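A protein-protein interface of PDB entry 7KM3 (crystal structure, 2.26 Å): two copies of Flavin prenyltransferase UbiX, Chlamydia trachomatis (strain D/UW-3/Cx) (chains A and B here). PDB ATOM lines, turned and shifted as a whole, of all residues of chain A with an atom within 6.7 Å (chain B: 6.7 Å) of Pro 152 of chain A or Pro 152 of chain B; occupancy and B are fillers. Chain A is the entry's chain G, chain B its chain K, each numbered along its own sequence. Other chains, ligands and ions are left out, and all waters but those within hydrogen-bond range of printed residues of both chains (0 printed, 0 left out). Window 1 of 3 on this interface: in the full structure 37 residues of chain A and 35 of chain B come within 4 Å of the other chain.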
ATOM      1  N   SER A  12     -32.097  -5.701 -23.035  1.00  0.00           N
ATOM      2  CA  SER A  12     -31.348  -5.676 -24.275  1.00  0.00           C
ATOM      3  C   SER A  12     -30.214  -6.702 -24.261  1.00  0.00           C
ATOM      4  O   SER A  12     -29.623  -6.998 -23.217  1.00  0.00           O
ATOM      5  CB  SER A  12     -30.785  -4.277 -24.517  1.00  0.00           C
ATOM      6  OG  SER A  12     -30.190  -4.200 -25.799  1.00  0.00           O
ATOM      7  N   LEU A  16     -27.214 -12.523 -26.808  1.00  0.00           N
ATOM      8  CA  LEU A  16     -26.399 -13.280 -25.862  1.00  0.00           C
ATOM      9  C   LEU A  16     -27.003 -14.649 -25.595  1.00  0.00           C
ATOM     10  O   LEU A  16     -26.288 -15.660 -25.571  1.00  0.00           O
ATOM     11  CB  LEU A  16     -26.228 -12.510 -24.556  1.00  0.00           C
ATOM     12  CG  LEU A  16     -25.521 -11.158 -24.629  1.00  0.00           C
ATOM     13  CD1 LEU A  16     -25.370 -10.573 -23.245  1.00  0.00           C
ATOM     14  CD2 LEU A  16     -24.167 -11.283 -25.318  1.00  0.00           C
ATOM     15  N   PRO A  90     -30.676 -12.286 -21.359  1.00  0.00           N
ATOM     16  CA  PRO A  90     -30.252 -11.192 -20.480  1.00  0.00           C
ATOM     17  C   PRO A  90     -31.188 -11.110 -19.288  1.00  0.00           C
ATOM     18  O   PRO A  90     -32.278 -11.634 -19.370  1.00  0.00           O
ATOM     19  CB  PRO A  90     -30.407  -9.932 -21.349  1.00  0.00           C
ATOM     20  CG  PRO A  90     -30.849 -10.383 -22.695  1.00  0.00           C
ATOM     21  CD  PRO A  90     -31.318 -11.798 -22.591  1.00  0.00           C
ATOM     22  N   VAL A 125     -27.276 -12.397 -15.897  1.00  0.00           N
ATOM     23  CA  VAL A 125     -26.578 -11.483 -16.792  1.00  0.00           C
ATOM     24  C   VAL A 125     -27.366 -10.180 -16.842  1.00  0.00           C
ATOM     25  O   VAL A 125     -28.073  -9.899 -17.829  1.00  0.00           O
ATOM     26  CB  VAL A 125     -26.369 -12.119 -18.175  1.00  0.00           C
ATOM     27  CG1 VAL A 125     -25.593 -11.175 -19.102  1.00  0.00           C
ATOM     28  CG2 VAL A 125     -25.616 -13.435 -18.015  1.00  0.00           C
ATOM     29  N   PRO A 126     -27.274  -9.359 -15.794  1.00  0.00           N
ATOM     30  CA  PRO A 126     -28.097  -8.148 -15.730  1.00  0.00           C
ATOM     31  C   PRO A 126     -27.565  -7.088 -16.671  1.00  0.00           C
ATOM     32  O   PRO A 126     -26.370  -6.782 -16.675  1.00  0.00           O
ATOM     33  CB  PRO A 126     -27.972  -7.709 -14.264  1.00  0.00           C
ATOM     34  CG  PRO A 126     -26.610  -8.176 -13.868  1.00  0.00           C
ATOM     35  CD  PRO A 126     -26.416  -9.500 -14.604  1.00  0.00           C
ATOM     36  N   ARG A 127     -28.465  -6.506 -17.452  1.00  0.00           N
ATOM     37  CA  ARG A 127     -28.133  -5.416 -18.356  1.00  0.00           C
ATOM     38  C   ARG A 127     -29.006  -4.214 -18.014  1.00  0.00           C
ATOM     39  O   ARG A 127     -30.231  -4.265 -18.181  1.00  0.00           O
ATOM     40  CB  ARG A 127     -28.332  -5.840 -19.806  1.00  0.00           C
ATOM     41  CG  ARG A 127     -27.649  -4.914 -20.757  1.00  0.00           C
ATOM     42  CD  ARG A 127     -28.594  -4.299 -21.753  1.00  0.00           C
ATOM     43  NE  ARG A 127     -27.953  -3.122 -22.310  1.00  0.00           N
ATOM     44  CZ  ARG A 127     -28.268  -1.872 -21.981  1.00  0.00           C
ATOM     45  NH1 ARG A 127     -29.257  -1.631 -21.123  1.00  0.00           N
ATOM     46  NH2 ARG A 127     -27.603  -0.866 -22.524  1.00  0.00           N
ATOM     47  N   GLU A 128     -28.380  -3.142 -17.538  1.00  0.00           N
ATOM     48  CA  GLU A 128     -29.057  -1.876 -17.295  1.00  0.00           C
ATOM     49  C   GLU A 128     -27.995  -0.826 -17.010  1.00  0.00           C
ATOM     50  O   GLU A 128     -26.993  -1.118 -16.355  1.00  0.00           O
ATOM     51  CB  GLU A 128     -30.044  -1.974 -16.113  1.00  0.00           C
ATOM     52  CG  GLU A 128     -30.741  -0.645 -15.737  1.00  0.00           C
ATOM     53  CD  GLU A 128     -31.660  -0.125 -16.847  1.00  0.00           C
ATOM     54  OE1 GLU A 128     -32.897  -0.217 -16.686  1.00  0.00           O
ATOM     55  OE2 GLU A 128     -31.147   0.366 -17.882  1.00  0.00           O
ATOM     56  N   ALA A 129     -28.234   0.395 -17.467  1.00  0.00           N
ATOM     57  CA  ALA A 129     -27.275   1.462 -17.179  1.00  0.00           C
ATOM     58  C   ALA A 129     -27.904   2.840 -17.340  1.00  0.00           C
ATOM     59  O   ALA A 129     -28.558   3.086 -18.336  1.00  0.00           O
ATOM     60  CB  ALA A 129     -26.053   1.322 -18.093  1.00  0.00           C
ATOM     61  N   LEU A 150     -22.995 -11.420 -13.417  1.00  0.00           N
ATOM     62  CA  LEU A 150     -22.142 -11.363 -14.604  1.00  0.00           C
ATOM     63  C   LEU A 150     -22.754 -10.396 -15.612  1.00  0.00           C
ATOM     64  O   LEU A 150     -23.386 -10.826 -16.581  1.00  0.00           O
ATOM     65  CB  LEU A 150     -21.985 -12.761 -15.211  1.00  0.00           C
ATOM     66  CG  LEU A 150     -20.977 -12.924 -16.356  1.00  0.00           C
ATOM     67  CD1 LEU A 150     -19.578 -12.842 -15.807  1.00  0.00           C
ATOM     68  CD2 LEU A 150     -21.187 -14.243 -17.083  1.00  0.00           C
ATOM     69  N   PRO A 151     -22.607  -9.087 -15.400  1.00  0.00           N
ATOM     70  CA  PRO A 151     -23.096  -8.140 -16.400  1.00  0.00           C
ATOM     71  C   PRO A 151     -22.366  -8.359 -17.709  1.00  0.00           C
ATOM     72  O   PRO A 151     -21.236  -8.881 -17.723  1.00  0.00           O
ATOM     73  CB  PRO A 151     -22.755  -6.771 -15.794  1.00  0.00           C
ATOM     74  CG  PRO A 151     -22.171  -7.056 -14.392  1.00  0.00           C
ATOM     75  CD  PRO A 151     -21.720  -8.463 -14.408  1.00  0.00           C
ATOM     76  N   PRO A 152     -22.960  -8.012 -18.808  1.00  0.00           N
ATOM     77  CA  PRO A 152     -22.277  -8.295 -20.089  1.00  0.00           C
ATOM     78  C   PRO A 152     -21.257  -7.216 -20.453  1.00  0.00           C
ATOM     79  O   PRO A 152     -21.492  -6.303 -21.235  1.00  0.00           O
ATOM     80  CB  PRO A 152     -23.442  -8.389 -21.079  1.00  0.00           C
ATOM     81  CG  PRO A 152     -24.533  -7.543 -20.483  1.00  0.00           C
ATOM     82  CD  PRO A 152     -24.339  -7.520 -18.985  1.00  0.00           C
ATOM     83  N   MET A 153     -20.064  -7.355 -19.868  1.00  0.00           N
ATOM     84  CA  MET A 153     -19.000  -6.364 -19.989  1.00  0.00           C
ATOM     85  C   MET A 153     -18.102  -6.725 -21.160  1.00  0.00           C
ATOM     86  O   MET A 153     -17.449  -7.778 -21.110  1.00  0.00           O
ATOM     87  CB  MET A 153     -18.164  -6.318 -18.712  1.00  0.00           C
ATOM     88  CG  MET A 153     -18.940  -6.186 -17.407  1.00  0.00           C
ATOM     89  SD  MET A 153     -19.204  -4.440 -17.075  1.00  0.00           S
ATOM     90  CE  MET A 153     -19.346  -4.348 -15.286  1.00  0.00           C
ATOM     91  N   PRO A 154     -18.030  -5.914 -22.218  1.00  0.00           N
ATOM     92  CA  PRO A 154     -17.129  -6.239 -23.336  1.00  0.00           C
ATOM     93  C   PRO A 154     -15.695  -6.456 -22.867  1.00  0.00           C
ATOM     94  O   PRO A 154     -15.172  -5.729 -22.017  1.00  0.00           O
ATOM     95  CB  PRO A 154     -17.245  -5.018 -24.261  1.00  0.00           C
ATOM     96  CG  PRO A 154     -18.611  -4.441 -23.956  1.00  0.00           C
ATOM     97  CD  PRO A 154     -18.954  -4.814 -22.540  1.00  0.00           C
ATOM     98  N   TRP A 156     -12.403  -6.065 -23.874  1.00  0.00           N
ATOM     99  CA  TRP A 156     -11.684  -5.366 -24.929  1.00  0.00           C
ATOM    100  C   TRP A 156     -10.235  -5.822 -25.073  1.00  0.00           C
ATOM    101  O   TRP A 156      -9.646  -5.582 -26.129  1.00  0.00           O
ATOM    102  CB  TRP A 156     -11.743  -3.855 -24.697  1.00  0.00           C
ATOM    103  CG  TRP A 156     -13.018  -3.224 -25.205  1.00  0.00           C
ATOM    104  CD1 TRP A 156     -13.356  -3.005 -26.506  1.00  0.00           C
ATOM    105  CD2 TRP A 156     -14.111  -2.729 -24.419  1.00  0.00           C
ATOM    106  NE1 TRP A 156     -14.592  -2.414 -26.585  1.00  0.00           N
ATOM    107  CE2 TRP A 156     -15.076  -2.229 -25.316  1.00  0.00           C
ATOM    108  CE3 TRP A 156     -14.372  -2.672 -23.044  1.00  0.00           C
ATOM    109  CZ2 TRP A 156     -16.286  -1.678 -24.886  1.00  0.00           C
ATOM    110  CZ3 TRP A 156     -15.581  -2.112 -22.613  1.00  0.00           C
ATOM    111  CH2 TRP A 156     -16.519  -1.625 -23.533  1.00  0.00           C
ATOM    112  N   ILE A 166     -17.773  -9.182 -29.675  1.00  0.00           N
ATOM    113  CA  ILE A 166     -18.037  -8.800 -28.290  1.00  0.00           C
ATOM    114  C   ILE A 166     -19.038  -9.764 -27.665  1.00  0.00           C
ATOM    115  O   ILE A 166     -18.817 -10.287 -26.567  1.00  0.00           O
ATOM    116  CB  ILE A 166     -18.502  -7.334 -28.227  1.00  0.00           C
ATOM    117  CG1 ILE A 166     -17.280  -6.419 -28.415  1.00  0.00           C
ATOM    118  CG2 ILE A 166     -19.264  -7.046 -26.918  1.00  0.00           C
ATOM    119  CD1 ILE A 166     -17.577  -5.029 -28.988  1.00  0.00           C
ATOM    120  N   ILE A 170     -18.337 -12.526 -24.445  1.00  0.00           N
ATOM    121  CA  ILE A 170     -19.181 -12.503 -23.249  1.00  0.00           C
ATOM    122  C   ILE A 170     -19.802 -13.874 -22.998  1.00  0.00           C
ATOM    123  O   ILE A 170     -19.774 -14.392 -21.877  1.00  0.00           O
ATOM    124  CB  ILE A 170     -20.265 -11.424 -23.388  1.00  0.00           C
ATOM    125  CG1 ILE A 170     -19.656 -10.034 -23.256  1.00  0.00           C
ATOM    126  CG2 ILE A 170     -21.372 -11.630 -22.364  1.00  0.00           C
ATOM    127  CD1 ILE A 170     -20.601  -8.947 -23.671  1.00  0.00           C
ATOM    128  N   SER B  12     -10.257  -2.871 -18.593  1.00  0.00           N
ATOM    129  CA  SER B  12     -10.319  -3.029 -20.041  1.00  0.00           C
ATOM    130  C   SER B  12     -11.306  -2.034 -20.661  1.00  0.00           C
ATOM    131  O   SER B  12     -12.408  -1.821 -20.149  1.00  0.00           O
ATOM    132  CB  SER B  12     -10.719  -4.461 -20.394  1.00  0.00           C
ATOM    133  OG  SER B  12     -10.717  -4.663 -21.803  1.00  0.00           O
ATOM    134  N   LEU B  16     -12.954   3.629 -24.725  1.00  0.00           N
ATOM    135  CA  LEU B  16     -14.033   4.505 -24.269  1.00  0.00           C
ATOM    136  C   LEU B  16     -13.488   5.848 -23.803  1.00  0.00           C
ATOM    137  O   LEU B  16     -14.123   6.889 -24.005  1.00  0.00           O
ATOM    138  CB  LEU B  16     -14.828   3.844 -23.130  1.00  0.00           C
ATOM    139  CG  LEU B  16     -15.434   2.460 -23.352  1.00  0.00           C
ATOM    140  CD1 LEU B  16     -16.079   1.958 -22.070  1.00  0.00           C
ATOM    141  CD2 LEU B  16     -16.440   2.448 -24.538  1.00  0.00           C
ATOM    142  N   PRO B  90     -12.050   3.875 -18.284  1.00  0.00           N
ATOM    143  CA  PRO B  90     -12.761   2.843 -17.533  1.00  0.00           C
ATOM    144  C   PRO B  90     -12.407   3.008 -16.069  1.00  0.00           C
ATOM    145  O   PRO B  90     -11.504   3.789 -15.740  1.00  0.00           O
ATOM    146  CB  PRO B  90     -12.202   1.529 -18.098  1.00  0.00           C
ATOM    147  CG  PRO B  90     -11.292   1.935 -19.233  1.00  0.00           C
ATOM    148  CD  PRO B  90     -10.870   3.330 -18.961  1.00  0.00           C
ATOM    149  N   VAL B 125     -17.404   4.426 -14.720  1.00  0.00           N
ATOM    150  CA  VAL B 125     -17.693   3.423 -15.741  1.00  0.00           C
ATOM    151  C   VAL B 125     -17.004   2.129 -15.312  1.00  0.00           C
ATOM    152  O   VAL B 125     -15.969   1.752 -15.889  1.00  0.00           O
ATOM    153  CB  VAL B 125     -17.258   3.915 -17.137  1.00  0.00           C
ATOM    154  CG1 VAL B 125     -17.677   2.925 -18.241  1.00  0.00           C
ATOM    155  CG2 VAL B 125     -17.867   5.300 -17.421  1.00  0.00           C
ATOM    156  N   PRO B 126     -17.525   1.429 -14.294  1.00  0.00           N
ATOM    157  CA  PRO B 126     -16.800   0.272 -13.743  1.00  0.00           C
ATOM    158  C   PRO B 126     -16.895  -0.905 -14.696  1.00  0.00           C
ATOM    159  O   PRO B 126     -17.979  -1.253 -15.175  1.00  0.00           O
ATOM    160  CB  PRO B 126     -17.534  -0.017 -12.430  1.00  0.00           C
ATOM    161  CG  PRO B 126     -18.986   0.339 -12.776  1.00  0.00           C
ATOM    162  CD  PRO B 126     -18.842   1.602 -13.646  1.00  0.00           C
ATOM    163  N   ARG B 127     -15.754  -1.512 -14.980  1.00  0.00           N
ATOM    164  CA  ARG B 127     -15.700  -2.682 -15.842  1.00  0.00           C
ATOM    165  C   ARG B 127     -15.092  -3.825 -15.038  1.00  0.00           C
ATOM    166  O   ARG B 127     -13.923  -3.758 -14.636  1.00  0.00           O
ATOM    167  CB  ARG B 127     -14.901  -2.392 -17.116  1.00  0.00           C
ATOM    168  CG  ARG B 127     -15.143  -3.412 -18.223  1.00  0.00           C
ATOM    169  CD  ARG B 127     -13.953  -4.338 -18.413  1.00  0.00           C
ATOM    170  NE  ARG B 127     -14.330  -5.560 -19.117  1.00  0.00           N
ATOM    171  CZ  ARG B 127     -14.269  -6.781 -18.587  1.00  0.00           C
ATOM    172  NH1 ARG B 127     -13.828  -6.955 -17.351  1.00  0.00           N
ATOM    173  NH2 ARG B 127     -14.644  -7.831 -19.295  1.00  0.00           N
ATOM    174  N   GLU B 128     -15.884  -4.861 -14.794  1.00  0.00           N
ATOM    175  CA  GLU B 128     -15.416  -6.080 -14.139  1.00  0.00           C
ATOM    176  C   GLU B 128     -16.520  -7.120 -14.235  1.00  0.00           C
ATOM    177  O   GLU B 128     -17.703  -6.777 -14.198  1.00  0.00           O
ATOM    178  CB  GLU B 128     -15.041  -5.821 -12.673  1.00  0.00           C
ATOM    179  CG  GLU B 128     -14.506  -7.016 -11.888  1.00  0.00           C
ATOM    180  CD  GLU B 128     -13.302  -7.681 -12.544  1.00  0.00           C
ATOM    181  OE1 GLU B 128     -13.505  -8.436 -13.522  1.00  0.00           O
ATOM    182  OE2 GLU B 128     -12.154  -7.445 -12.095  1.00  0.00           O
ATOM    183  N   ALA B 129     -16.127  -8.386 -14.382  1.00  0.00           N
ATOM    184  CA  ALA B 129     -17.086  -9.498 -14.390  1.00  0.00           C
ATOM    185  C   ALA B 129     -16.431 -10.843 -14.041  1.00  0.00           C
ATOM    186  O   ALA B 129     -15.368 -11.164 -14.556  1.00  0.00           O
ATOM    187  CB  ALA B 129     -17.778  -9.591 -15.740  1.00  0.00           C
ATOM    188  N   LEU B 150     -22.254   3.690 -14.216  1.00  0.00           N
ATOM    189  CA  LEU B 150     -22.569   3.435 -15.622  1.00  0.00           C
ATOM    190  C   LEU B 150     -21.601   2.387 -16.164  1.00  0.00           C
ATOM    191  O   LEU B 150     -20.611   2.715 -16.833  1.00  0.00           O
ATOM    192  CB  LEU B 150     -22.527   4.730 -16.432  1.00  0.00           C
ATOM    193  CG  LEU B 150     -22.827   4.636 -17.931  1.00  0.00           C
ATOM    194  CD1 LEU B 150     -24.303   4.352 -18.183  1.00  0.00           C
ATOM    195  CD2 LEU B 150     -22.438   5.934 -18.573  1.00  0.00           C
ATOM    196  N   PRO B 151     -21.853   1.110 -15.881  1.00  0.00           N
ATOM    197  CA  PRO B 151     -21.036   0.063 -16.484  1.00  0.00           C
ATOM    198  C   PRO B 151     -21.177   0.089 -17.992  1.00  0.00           C
ATOM    199  O   PRO B 151     -22.224   0.500 -18.532  1.00  0.00           O
ATOM    200  CB  PRO B 151     -21.610  -1.227 -15.882  1.00  0.00           C
ATOM    201  CG  PRO B 151     -22.950  -0.852 -15.306  1.00  0.00           C
ATOM    202  CD  PRO B 151     -22.931   0.598 -15.014  1.00  0.00           C
ATOM    203  N   PRO B 152     -20.129  -0.312 -18.723  1.00  0.00           N
ATOM    204  CA  PRO B 152     -20.198  -0.312 -20.193  1.00  0.00           C
ATOM    205  C   PRO B 152     -21.063  -1.430 -20.765  1.00  0.00           C
ATOM    206  O   PRO B 152     -20.543  -2.422 -21.288  1.00  0.00           O
ATOM    207  CB  PRO B 152     -18.730  -0.478 -20.602  1.00  0.00           C
ATOM    208  CG  PRO B 152     -18.096  -1.188 -19.440  1.00  0.00           C
ATOM    209  CD  PRO B 152     -18.762  -0.582 -18.236  1.00  0.00           C
ATOM    210  N   MET B 153     -22.379  -1.270 -20.671  1.00  0.00           N
ATOM    211  CA  MET B 153     -23.342  -2.242 -21.187  1.00  0.00           C
ATOM    212  C   MET B 153     -23.630  -1.962 -22.658  1.00  0.00           C
ATOM    213  O   MET B 153     -24.144  -0.884 -22.975  1.00  0.00           O
ATOM    214  CB  MET B 153     -24.652  -2.150 -20.416  1.00  0.00           C
ATOM    215  CG  MET B 153     -24.558  -2.170 -18.892  1.00  0.00           C
ATOM    216  SD  MET B 153     -24.319  -3.840 -18.328  1.00  0.00           S
ATOM    217  CE  MET B 153     -24.862  -3.754 -16.595  1.00  0.00           C
ATOM    218  N   PRO B 154     -23.362  -2.890 -23.575  1.00  0.00           N
ATOM    219  CA  PRO B 154     -23.732  -2.644 -24.973  1.00  0.00           C
ATOM    220  C   PRO B 154     -25.239  -2.457 -25.136  1.00  0.00           C
ATOM    221  O   PRO B 154     -26.055  -3.151 -24.511  1.00  0.00           O
ATOM    222  CB  PRO B 154     -23.227  -3.897 -25.706  1.00  0.00           C
ATOM    223  CG  PRO B 154     -22.168  -4.445 -24.814  1.00  0.00           C
ATOM    224  CD  PRO B 154     -22.639  -4.162 -23.415  1.00  0.00           C
ATOM    225  N   TRP B 156     -27.842  -3.130 -27.471  1.00  0.00           N
ATOM    226  CA  TRP B 156     -28.072  -3.928 -28.669  1.00  0.00           C
ATOM    227  C   TRP B 156     -29.293  -3.475 -29.475  1.00  0.00           C
ATOM    228  O   TRP B 156     -29.382  -3.810 -30.663  1.00  0.00           O
ATOM    229  CB  TRP B 156     -28.185  -5.407 -28.302  1.00  0.00           C
ATOM    230  CG  TRP B 156     -26.839  -6.099 -28.151  1.00  0.00           C
ATOM    231  CD1 TRP B 156     -26.050  -6.584 -29.158  1.00  0.00           C
ATOM    232  CD2 TRP B 156     -26.145  -6.387 -26.929  1.00  0.00           C
ATOM    233  NE1 TRP B 156     -24.906  -7.145 -28.639  1.00  0.00           N
ATOM    234  CE2 TRP B 156     -24.946  -7.043 -27.273  1.00  0.00           C
ATOM    235  CE3 TRP B 156     -26.420  -6.145 -25.578  1.00  0.00           C
ATOM    236  CZ2 TRP B 156     -24.028  -7.472 -26.313  1.00  0.00           C
ATOM    237  CZ3 TRP B 156     -25.513  -6.580 -24.624  1.00  0.00           C
ATOM    238  CH2 TRP B 156     -24.327  -7.230 -24.999  1.00  0.00           C
ATOM    239  N   ILE B 166     -20.343  -0.258 -30.811  1.00  0.00           N
ATOM    240  CA  ILE B 166     -20.726  -0.500 -29.422  1.00  0.00           C
ATOM    241  C   ILE B 166     -20.010   0.469 -28.492  1.00  0.00           C
ATOM    242  O   ILE B 166     -20.624   1.035 -27.585  1.00  0.00           O
ATOM    243  CB  ILE B 166     -20.477  -1.969 -29.039  1.00  0.00           C
ATOM    244  CG1 ILE B 166     -21.583  -2.840 -29.637  1.00  0.00           C
ATOM    245  CG2 ILE B 166     -20.405  -2.130 -27.522  1.00  0.00           C
ATOM    246  CD1 ILE B 166     -21.375  -4.319 -29.490  1.00  0.00           C
ATOM    247  N   ILE B 170     -21.971   3.524 -26.181  1.00  0.00           N
ATOM    248  CA  ILE B 170     -21.704   3.620 -24.747  1.00  0.00           C
ATOM    249  C   ILE B 170     -21.237   5.024 -24.383  1.00  0.00           C
ATOM    250  O   ILE B 170     -21.681   5.610 -23.389  1.00  0.00           O
ATOM    251  CB  ILE B 170     -20.676   2.543 -24.344  1.00  0.00           C
ATOM    252  CG1 ILE B 170     -21.322   1.159 -24.360  1.00  0.00           C
ATOM    253  CG2 ILE B 170     -20.013   2.848 -22.983  1.00  0.00           C
ATOM    254  CD1 ILE B 170     -20.309   0.033 -24.426  1.00  0.00           C
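Hydrophobic or aromatic side chains of chain B that line the printed part of chain A: Leu 16, Ala 129, Leu 150, Pro 151, Pro 152, Met 153, Pro 154, Trp 156 and Ile 166. Of the 16 printed residues of chain A, 13 touch a printed residue of chain B.
Pro 152 of chain A touches Pro 154 of chain B, and with the chains exchanged Pro 154 of chain A touches Pro 152 of chain B. Pro 154 of chain B touches its own counterpart, Pro 154 of chain A. Trp 156 of chain A touches Pro 152 of chain B, but with the chains exchanged Pro 152 of chain A does not touch Trp 156 of chain B (4.2 Å). Ile 166 of chain B touches its own counterpart, Ile 166 of chain A. Of the 26 pairs that touch across the chains among the printed residues, 23 have their exchanged pair printed and touching as well.
CD1 of Leu 16 of chain A touches CH2 of Trp 156 of chain B, at 3.9 Å. Met 153 of chain B touches Pro 126 of chain A. Ala 129 of chain A touches Leu 150 of chain B (CB to CD1, 3.5 Å). CB of Ala 129 of chain A touches O of Pro 151 of chain B (3.9 Å). CD1 of Leu 150 of chain A touches CB of Ala 129 of chain B, 3.7 Å away. Pro 151 of chain A touches Met 153 of chain B. CE of Met 153 of chain A touches O of Pro 126 of chain B, 3.4 Å away. Pro 154 of chain B touches Pro 154 of chain A (CG to CG, 3.7 Å). CH2 of Trp 156 of chain A touches CB of Pro 152 of chain B, 3.8 Å away. CD1 of Ile 166 of chain A touches CD1 of Ile 166 of chain B, 3.9 Å away.
The guanidinium group (NH2) of Arg 127 of chain A is in hydrogen-bond range of the backbone carbonyl oxygen (O) of Met 153 of chain B (3.5 Å). O of Met 153 of chain A is in hydrogen-bond range of NH2 of Arg 127 of chain B, 3.3 Å away. O of Pro 154 of chain A sits at hydrogen-bond distance from NE of Arg 127 of chain B (3.0 Å). The side-chain hydroxyl (OG) of Ser 12 of chain A is in hydrogen-bond range of the backbone NH (N) of Trp 156 of chain B (3.1 Å). OG of Ser 12 of chain B sits at hydrogen-bond distance from N of Trp 156 of chain A (3.0 Å). The backbone carbonyl oxygen (O) of Pro 154 of chain B lies within hydrogen-bond range of the guanidinium group (NE) of Arg 127 of chain A.
Of the printed residues of chain B, Pro 152 of chain A touches Pro 152 (3.996 Å), Met 153 (3.7 Å) and Pro 154 (3.3 Å). Of the printed residues of chain B, Met 153 of chain A touches Pro 126, Arg 127, Glu 128, Ala 129 and Pro 151. Printed residues of chain B within 4 Å of Pro 154 of chain A: Arg 127 (3.0 Å), Pro 152 (3.1 Å) and Pro 154 (3.7 Å). Printed residues of chain B within 4 Å of Trp 156 of chain A: Ser 12 (3.0 Å), Leu 16 (3.9 Å) and Pro 152 (3.8 Å). Of the printed residues of chain A, Pro 151 of chain B touches Ala 129 (3.9 Å) and Met 153 (3.9 Å). Printed residues of chain A within 4 Å of Met 153 of chain B: Pro 126, Arg 127, Glu 128, Ala 129, Pro 151 and Pro 152. Val 125 of chain B touches none of the printed residues of chain A. The nearest printed residue of chain A that does not touch Pro 152 of chain B is Met 153 of chain A (4.1 Å). The nearest printed residue of chain B that does not touch Ile 166 of chain A is Pro 154 of chain B (4.4 Å).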
